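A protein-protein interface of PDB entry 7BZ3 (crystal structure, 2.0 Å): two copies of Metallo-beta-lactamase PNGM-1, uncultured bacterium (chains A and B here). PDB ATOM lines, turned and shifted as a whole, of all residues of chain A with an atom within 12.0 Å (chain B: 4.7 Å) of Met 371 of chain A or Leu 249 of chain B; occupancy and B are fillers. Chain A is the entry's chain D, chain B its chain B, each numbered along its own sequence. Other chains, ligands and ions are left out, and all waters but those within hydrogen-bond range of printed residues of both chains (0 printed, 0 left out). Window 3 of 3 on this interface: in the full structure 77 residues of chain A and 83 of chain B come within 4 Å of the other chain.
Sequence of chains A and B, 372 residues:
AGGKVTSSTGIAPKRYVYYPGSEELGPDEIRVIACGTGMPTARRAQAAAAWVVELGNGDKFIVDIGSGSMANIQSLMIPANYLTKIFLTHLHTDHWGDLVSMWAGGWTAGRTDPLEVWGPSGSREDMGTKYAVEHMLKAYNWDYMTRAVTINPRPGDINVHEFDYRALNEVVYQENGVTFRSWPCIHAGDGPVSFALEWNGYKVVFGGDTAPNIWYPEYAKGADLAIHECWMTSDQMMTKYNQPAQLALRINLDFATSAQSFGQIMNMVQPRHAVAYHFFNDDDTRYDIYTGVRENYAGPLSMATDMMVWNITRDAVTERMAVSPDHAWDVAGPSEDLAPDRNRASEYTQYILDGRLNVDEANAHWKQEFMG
Among the printed residues, pairs that only touch across the chains: Trp 366 of chain A with Ser 234 of chain B (3.1 Å), Phe 370 of chain A with Ala 245 of chain B (3.5 Å), Trp 366 of chain A with Asn 252 of chain B (3.5 Å), Trp 366 of chain A with Leu 249 of chain B (3.5 Å), Phe 370 of chain A with Ser 234 of chain B (3.6 Å), Lys 367 of chain A with Leu 249 of chain B (3.6 Å), Lys 367 of chain A with Arg 250 of chain B (3.7 Å), Lys 367 of chain A with Leu 253 of chain B (3.8 Å), Asn 363 of chain A with Asn 252 of chain B (3.8 Å), Met 371 of chain A with Leu 249 of chain B (3.9 Å) and Phe 370 of chain A with Ala 248 of chain B (3.98 Å).
Of the 14 printed residues of chain A, 5 touch a printed residue of chain B.
Of the 10 printed residues of chain B, 7 touch a printed residue of chain A.
Hydrophobic or aromatic side chains of chain B that line the printed part of chain A: Ala 245, Ala 248, Leu 249 and Leu 253.
Among the printed residues, 11 pairs touch across the chains.
The side-chain amide oxygen of Asn 363 of chain A lies within hydrogen-bond range of the indole nitrogen of Trp 366 of chain A, at 3.0 Å.
The backbone carbonyl oxygen of Val 359 of chain A is in hydrogen-bond range of the side-chain amide nitrogen of Asn 363 of chain A, at 2.7 Å.
The side-chain hydroxyl of Ser 234 of chain B sits at hydrogen-bond distance from the backbone carbonyl oxygen of Ala 248 of chain B, at 2.7 Å.
The backbone NH (N) of Ser 234 of chain B lies close to the side-chain amide nitrogen (ND2) of Asn 252 of chain B (2.9 Å).
Of chain A, only Trp 366, Lys 367 and Met 371 come within 4 Å of Leu 249 of chain B.
Ser 234 of chain B touches two residues of chain A.
Gln 246 of chain B touches none of the printed residues of chain A.
Of chain A, only Lys 367 comes within 4 Å of Arg 250 of chain B.
No residue of chain A comes within 4 Å of Ile 251 of chain B.
Of chain A, only Asn 363 and Trp 366 come within 4 Å of Asn 252 of chain B.
Printed residues of chain B within 4 Å of Trp 366 of chain A: Ser 234, Leu 249 and Asn 252.
Printed residues of chain B within 4 Å of Lys 367 of chain A: Leu 249, Arg 250 and Leu 253.
Printed residues of chain B within 4 Å of Phe 370 of chain A: Ser 234 (3.6 Å), Ala 245 (3.5 Å) and Ala 248 (3.98 Å).
Arg 356 of chain A touches none of the printed residues of chain B.
The nearest printed residue of chain B that does not touch Met 371 of chain A is Ala 245 of chain B (6.4 Å).
The nearest residue of chain A that does not touch Leu 249 of chain B is Phe 370 of chain A (4.3 Å).
No position is printed for both chains.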
ATOM      1  N   ARG A 356      -4.326  15.309 -22.916  1.00  0.00           N
ATOM      2  CA  ARG A 356      -4.940  13.957 -23.088  1.00  0.00           C
ATOM      3  C   ARG A 356      -4.465  13.005 -21.982  1.00  0.00           C
ATOM      4  O   ARG A 356      -3.281  12.886 -21.805  1.00  0.00           O
ATOM      5  CB  ARG A 356      -4.631  13.369 -24.470  1.00  0.00           C
ATOM      6  CG  ARG A 356      -5.574  13.855 -25.559  1.00  0.00           C
ATOM      7  CD  ARG A 356      -5.865  12.862 -26.669  1.00  0.00           C
ATOM      8  NE  ARG A 356      -6.880  13.398 -27.580  1.00  0.00           N
ATOM      9  CZ  ARG A 356      -8.206  13.181 -27.509  1.00  0.00           C
ATOM     10  NH1 ARG A 356      -8.720  12.410 -26.564  1.00  0.00           N
ATOM     11  NH2 ARG A 356      -9.018  13.727 -28.405  1.00  0.00           N
ATOM     12  N   VAL A 359      -5.355   6.344 -21.587  1.00  0.00           N
ATOM     13  CA  VAL A 359      -6.403   5.427 -21.055  1.00  0.00           C
ATOM     14  C   VAL A 359      -6.290   4.059 -21.756  1.00  0.00           C
ATOM     15  O   VAL A 359      -7.345   3.443 -22.061  1.00  0.00           O
ATOM     16  CB  VAL A 359      -7.809   6.046 -21.223  1.00  0.00           C
ATOM     17  CG1 VAL A 359      -8.014   7.282 -20.348  1.00  0.00           C
ATOM     18  CG2 VAL A 359      -8.142   6.371 -22.666  1.00  0.00           C
ATOM     19  N   ASP A 360      -5.062   3.579 -21.985  1.00  0.00           N
ATOM     20  CA  ASP A 360      -4.776   2.363 -22.799  1.00  0.00           C
ATOM     21  C   ASP A 360      -5.068   1.107 -21.964  1.00  0.00           C
ATOM     22  O   ASP A 360      -5.876   0.294 -22.429  1.00  0.00           O
ATOM     23  CB  ASP A 360      -3.333   2.370 -23.330  1.00  0.00           C
ATOM     24  CG  ASP A 360      -3.103   3.219 -24.571  1.00  0.00           C
ATOM     25  OD1 ASP A 360      -4.101   3.693 -25.171  1.00  0.00           O
ATOM     26  OD2 ASP A 360      -1.929   3.393 -24.940  1.00  0.00           O
ATOM     27  N   ALA A 362      -6.929   0.759 -19.365  1.00  0.00           N
ATOM     28  CA  ALA A 362      -8.357   0.730 -18.961  1.00  0.00           C
ATOM     29  C   ALA A 362      -9.248   0.266 -20.118  1.00  0.00           C
ATOM     30  O   ALA A 362     -10.326  -0.305 -19.875  1.00  0.00           O
ATOM     31  CB  ALA A 362      -8.754   2.110 -18.496  1.00  0.00           C
ATOM     32  N   ASN A 363      -8.858   0.553 -21.351  1.00  0.00           N
ATOM     33  CA  ASN A 363      -9.736   0.360 -22.531  1.00  0.00           C
ATOM     34  C   ASN A 363      -9.297  -0.884 -23.330  1.00  0.00           C
ATOM     35  O   ASN A 363     -10.010  -1.200 -24.308  1.00  0.00           O
ATOM     36  CB  ASN A 363      -9.823   1.638 -23.375  1.00  0.00           C
ATOM     37  CG  ASN A 363     -10.670   2.718 -22.730  1.00  0.00           C
ATOM     38  OD1 ASN A 363     -11.858   2.858 -23.037  1.00  0.00           O
ATOM     39  ND2 ASN A 363     -10.081   3.475 -21.819  1.00  0.00           N
ATOM     40  N   ALA A 364      -8.242  -1.596 -22.906  1.00  0.00           N
ATOM     41  CA  ALA A 364      -7.645  -2.745 -23.641  1.00  0.00           C
ATOM     42  C   ALA A 364      -8.626  -3.931 -23.701  1.00  0.00           C
ATOM     43  O   ALA A 364      -8.908  -4.396 -24.795  1.00  0.00           O
ATOM     44  CB  ALA A 364      -6.333  -3.151 -23.016  1.00  0.00           C
ATOM     45  N   HIS A 365      -9.157  -4.377 -22.563  1.00  0.00           N
ATOM     46  CA  HIS A 365     -10.033  -5.578 -22.449  1.00  0.00           C
ATOM     47  C   HIS A 365     -11.278  -5.441 -23.344  1.00  0.00           C
ATOM     48  O   HIS A 365     -11.521  -6.376 -24.128  1.00  0.00           O
ATOM     49  CB  HIS A 365     -10.378  -5.862 -20.980  1.00  0.00           C
ATOM     50  CG  HIS A 365     -11.102  -7.150 -20.754  1.00  0.00           C
ATOM     51  ND1 HIS A 365     -12.451  -7.307 -21.039  1.00  0.00           N
ATOM     52  CD2 HIS A 365     -10.683  -8.328 -20.242  1.00  0.00           C
ATOM     53  CE1 HIS A 365     -12.829  -8.525 -20.715  1.00  0.00           C
ATOM     54  NE2 HIS A 365     -11.761  -9.174 -20.228  1.00  0.00           N
ATOM     55  N   TRP A 366     -12.050  -4.346 -23.243  1.00  0.00           N
ATOM     56  CA  TRP A 366     -13.267  -4.139 -24.076  1.00  0.00           C
ATOM     57  C   TRP A 366     -12.860  -4.057 -25.552  1.00  0.00           C
ATOM     58  O   TRP A 366     -13.636  -4.527 -26.412  1.00  0.00           O
ATOM     59  CB  TRP A 366     -14.114  -2.930 -23.607  1.00  0.00           C
ATOM     60  CG  TRP A 366     -13.845  -1.567 -24.188  1.00  0.00           C
ATOM     61  CD1 TRP A 366     -13.175  -0.542 -23.585  1.00  0.00           C
ATOM     62  CD2 TRP A 366     -14.361  -1.018 -25.413  1.00  0.00           C
ATOM     63  NE1 TRP A 366     -13.181   0.575 -24.377  1.00  0.00           N
ATOM     64  CE2 TRP A 366     -13.886   0.312 -25.510  1.00  0.00           C
ATOM     65  CE3 TRP A 366     -15.126  -1.528 -26.458  1.00  0.00           C
ATOM     66  CZ2 TRP A 366     -14.153   1.136 -26.596  1.00  0.00           C
ATOM     67  CZ3 TRP A 366     -15.405  -0.713 -27.531  1.00  0.00           C
ATOM     68  CH2 TRP A 366     -14.913   0.592 -27.603  1.00  0.00           C
ATOM     69  N   LYS A 367     -11.684  -3.481 -25.807  1.00  0.00           N
ATOM     70  CA  LYS A 367     -11.124  -3.214 -27.160  1.00  0.00           C
ATOM     71  C   LYS A 367     -10.801  -4.536 -27.861  1.00  0.00           C
ATOM     72  O   LYS A 367     -11.126  -4.650 -29.050  1.00  0.00           O
ATOM     73  CB  LYS A 367      -9.850  -2.374 -27.050  1.00  0.00           C
ATOM     74  CG  LYS A 367      -9.406  -1.675 -28.322  1.00  0.00           C
ATOM     75  CD  LYS A 367      -8.180  -0.817 -28.110  1.00  0.00           C
ATOM     76  CE  LYS A 367      -7.554  -0.379 -29.413  1.00  0.00           C
ATOM     77  NZ  LYS A 367      -8.565   0.195 -30.333  1.00  0.00           N
ATOM     78  N   GLN A 368     -10.209  -5.494 -27.138  1.00  0.00           N
ATOM     79  CA  GLN A 368      -9.787  -6.814 -27.682  1.00  0.00           C
ATOM     80  C   GLN A 368     -11.023  -7.718 -27.935  1.00  0.00           C
ATOM     81  O   GLN A 368     -10.866  -8.726 -28.666  1.00  0.00           O
ATOM     82  CB  GLN A 368      -8.720  -7.369 -26.733  1.00  0.00           C
ATOM     83  CG  GLN A 368      -7.987  -8.602 -27.235  1.00  0.00           C
ATOM     84  CD  GLN A 368      -7.368  -9.368 -26.088  1.00  0.00           C
ATOM     85  OE1 GLN A 368      -7.883 -10.401 -25.649  1.00  0.00           O
ATOM     86  NE2 GLN A 368      -6.259  -8.853 -25.576  1.00  0.00           N
ATOM     87  N   GLU A 369     -12.211  -7.374 -27.397  1.00  0.00           N
ATOM     88  CA  GLU A 369     -13.529  -8.036 -27.674  1.00  0.00           C
ATOM     89  C   GLU A 369     -14.224  -7.389 -28.877  1.00  0.00           C
ATOM     90  O   GLU A 369     -14.760  -8.130 -29.735  1.00  0.00           O
ATOM     91  CB  GLU A 369     -14.488  -7.891 -26.490  1.00  0.00           C
ATOM     92  CG  GLU A 369     -15.748  -8.753 -26.568  1.00  0.00           C
ATOM     93  CD  GLU A 369     -16.965  -8.260 -27.358  1.00  0.00           C
ATOM     94  OE1 GLU A 369     -17.278  -7.019 -27.348  1.00  0.00           O
ATOM     95  OE2 GLU A 369     -17.640  -9.141 -27.972  1.00  0.00           O
ATOM     96  N   PHE A 370     -14.271  -6.052 -28.904  1.00  0.00           N
ATOM     97  CA  PHE A 370     -15.034  -5.249 -29.895  1.00  0.00           C
ATOM     98  C   PHE A 370     -14.401  -5.360 -31.283  1.00  0.00           C
ATOM     99  O   PHE A 370     -15.144  -5.401 -32.295  1.00  0.00           O
ATOM    100  CB  PHE A 370     -15.089  -3.766 -29.522  1.00  0.00           C
ATOM    101  CG  PHE A 370     -16.014  -3.030 -30.447  1.00  0.00           C
ATOM    102  CD1 PHE A 370     -15.587  -2.669 -31.714  1.00  0.00           C
ATOM    103  CD2 PHE A 370     -17.349  -2.847 -30.119  1.00  0.00           C
ATOM    104  CE1 PHE A 370     -16.457  -2.070 -32.605  1.00  0.00           C
ATOM    105  CE2 PHE A 370     -18.211  -2.219 -30.997  1.00  0.00           C
ATOM    106  CZ  PHE A 370     -17.765  -1.823 -32.235  1.00  0.00           C
ATOM    107  N   MET A 371     -13.066  -5.302 -31.320  1.00  0.00           N
ATOM    108  CA  MET A 371     -12.225  -5.525 -32.530  1.00  0.00           C
ATOM    109  C   MET A 371     -12.408  -6.974 -33.011  1.00  0.00           C
ATOM    110  O   MET A 371     -12.132  -7.222 -34.201  1.00  0.00           O
ATOM    111  CB  MET A 371     -10.744  -5.237 -32.234  1.00  0.00           C
ATOM    112  CG  MET A 371     -10.426  -3.750 -32.042  1.00  0.00           C
ATOM    113  SD  MET A 371      -8.698  -3.397 -31.590  1.00  0.00           S
ATOM    114  CE  MET A 371      -7.923  -3.378 -33.207  1.00  0.00           C
ATOM    115  N   GLY A 372     -12.846  -7.878 -32.119  1.00  0.00           N
ATOM    116  CA  GLY A 372     -13.401  -9.212 -32.444  1.00  0.00           C
ATOM    117  C   GLY A 372     -14.926  -9.208 -32.500  1.00  0.00           C
ATOM    118  O   GLY A 372     -15.608  -8.651 -33.375  1.00  0.00           O
ATOM    119  N   SER B 234     -19.733   1.453 -27.558  1.00  0.00           N
ATOM    120  CA  SER B 234     -19.527   1.320 -29.019  1.00  0.00           C
ATOM    121  C   SER B 234     -20.527   0.274 -29.548  1.00  0.00           C
ATOM    122  O   SER B 234     -21.227   0.564 -30.552  1.00  0.00           O
ATOM    123  CB  SER B 234     -18.107   0.990 -29.313  1.00  0.00           C
ATOM    124  OG  SER B 234     -17.272   2.079 -28.967  1.00  0.00           O
ATOM    125  N   ALA B 245     -17.963  -0.575 -36.892  1.00  0.00           N
ATOM    126  CA  ALA B 245     -16.975  -0.939 -35.846  1.00  0.00           C
ATOM    127  C   ALA B 245     -15.856   0.115 -35.823  1.00  0.00           C
ATOM    128  O   ALA B 245     -15.488   0.559 -34.713  1.00  0.00           O
ATOM    129  CB  ALA B 245     -16.442  -2.335 -36.090  1.00  0.00           C
ATOM    130  N   GLN B 246     -15.359   0.490 -37.012  1.00  0.00           N
ATOM    131  CA  GLN B 246     -14.509   1.686 -37.287  1.00  0.00           C
ATOM    132  C   GLN B 246     -14.941   2.841 -36.370  1.00  0.00           C
ATOM    133  O   GLN B 246     -14.333   2.982 -35.293  1.00  0.00           O
ATOM    134  CB  GLN B 246     -14.583   2.033 -38.786  1.00  0.00           C
ATOM    135  CG  GLN B 246     -14.268   3.483 -39.161  1.00  0.00           C
ATOM    136  CD  GLN B 246     -12.800   3.850 -39.164  1.00  0.00           C
ATOM    137  OE1 GLN B 246     -11.954   3.147 -39.723  1.00  0.00           O
ATOM    138  NE2 GLN B 246     -12.493   5.000 -38.582  1.00  0.00           N
ATOM    139  N   LEU B 247     -15.982   3.595 -36.752  1.00  0.00           N
ATOM    140  CA  LEU B 247     -16.264   4.949 -36.207  1.00  0.00           C
ATOM    141  C   LEU B 247     -16.882   4.835 -34.809  1.00  0.00           C
ATOM    142  O   LEU B 247     -16.944   5.867 -34.103  1.00  0.00           O
ATOM    143  CB  LEU B 247     -17.176   5.703 -37.179  1.00  0.00           C
ATOM    144  CG  LEU B 247     -16.903   7.205 -37.312  1.00  0.00           C
ATOM    145  CD1 LEU B 247     -15.410   7.535 -37.271  1.00  0.00           C
ATOM    146  CD2 LEU B 247     -17.515   7.745 -38.599  1.00  0.00           C
ATOM    147  N   ALA B 248     -17.305   3.618 -34.440  1.00  0.00           N
ATOM    148  CA  ALA B 248     -17.931   3.249 -33.151  1.00  0.00           C
ATOM    149  C   ALA B 248     -16.869   3.183 -32.068  1.00  0.00           C
ATOM    150  O   ALA B 248     -17.049   3.847 -31.011  1.00  0.00           O
ATOM    151  CB  ALA B 248     -18.630   1.917 -33.287  1.00  0.00           C
ATOM    152  N   LEU B 249     -15.854   2.353 -32.327  1.00  0.00           N
ATOM    153  CA  LEU B 249     -14.636   2.188 -31.497  1.00  0.00           C
ATOM    154  C   LEU B 249     -13.974   3.561 -31.312  1.00  0.00           C
ATOM    155  O   LEU B 249     -13.406   3.796 -30.233  1.00  0.00           O
ATOM    156  CB  LEU B 249     -13.716   1.188 -32.206  1.00  0.00           C
ATOM    157  CG  LEU B 249     -12.358   0.918 -31.557  1.00  0.00           C
ATOM    158  CD1 LEU B 249     -12.503   0.320 -30.160  1.00  0.00           C
ATOM    159  CD2 LEU B 249     -11.520   0.012 -32.448  1.00  0.00           C
ATOM    160  N   ARG B 250     -14.076   4.441 -32.314  1.00  0.00           N
ATOM    161  CA  ARG B 250     -13.367   5.755 -32.328  1.00  0.00           C
ATOM    162  C   ARG B 250     -13.972   6.637 -31.241  1.00  0.00           C
ATOM    163  O   ARG B 250     -13.203   7.171 -30.409  1.00  0.00           O
ATOM    164  CB  ARG B 250     -13.438   6.464 -33.692  1.00  0.00           C
ATOM    165  CG  ARG B 250     -12.438   5.951 -34.715  1.00  0.00           C
ATOM    166  CD  ARG B 250     -11.020   5.880 -34.169  1.00  0.00           C
ATOM    167  NE  ARG B 250     -10.704   4.683 -33.389  1.00  0.00           N
ATOM    168  CZ  ARG B 250      -9.596   4.512 -32.653  1.00  0.00           C
ATOM    169  NH1 ARG B 250      -8.672   5.459 -32.592  1.00  0.00           N
ATOM    170  NH2 ARG B 250      -9.418   3.393 -31.970  1.00  0.00           N
ATOM    171  N   ILE B 251     -15.297   6.742 -31.236  1.00  0.00           N
ATOM    172  CA  ILE B 251     -16.037   7.601 -30.275  1.00  0.00           C
ATOM    173  C   ILE B 251     -15.591   7.256 -28.844  1.00  0.00           C
ATOM    174  O   ILE B 251     -15.272   8.204 -28.095  1.00  0.00           O
ATOM    175  CB  ILE B 251     -17.556   7.487 -30.488  1.00  0.00           C
ATOM    176  CG1 ILE B 251     -17.948   8.002 -31.882  1.00  0.00           C
ATOM    177  CG2 ILE B 251     -18.281   8.218 -29.370  1.00  0.00           C
ATOM    178  CD1 ILE B 251     -19.438   8.168 -32.114  1.00  0.00           C
ATOM    179  N   ASN B 252     -15.496   5.969 -28.484  1.00  0.00           N
ATOM    180  CA  ASN B 252     -15.191   5.530 -27.089  1.00  0.00           C
ATOM    181  C   ASN B 252     -13.675   5.438 -26.846  1.00  0.00           C
ATOM    182  O   ASN B 252     -13.295   5.217 -25.680  1.00  0.00           O
ATOM    183  CB  ASN B 252     -15.870   4.210 -26.714  1.00  0.00           C
ATOM    184  CG  ASN B 252     -17.226   4.402 -26.067  1.00  0.00           C
ATOM    185  OD1 ASN B 252     -17.400   5.226 -25.164  1.00  0.00           O
ATOM    186  ND2 ASN B 252     -18.196   3.649 -26.541  1.00  0.00           N
ATOM    187  N   LEU B 253     -12.847   5.588 -27.884  1.00  0.00           N
ATOM    188  CA  LEU B 253     -11.363   5.553 -27.771  1.00  0.00           C
ATOM    189  C   LEU B 253     -10.768   6.964 -27.840  1.00  0.00           C
ATOM    190  O   LEU B 253      -9.795   7.200 -27.124  1.00  0.00           O
ATOM    191  CB  LEU B 253     -10.787   4.681 -28.890  1.00  0.00           C
ATOM    192  CG  LEU B 253      -9.703   3.696 -28.462  1.00  0.00           C
ATOM    193  CD1 LEU B 253      -8.699   4.344 -27.510  1.00  0.00           C
ATOM    194  CD2 LEU B 253     -10.322   2.463 -27.830  1.00  0.00           C
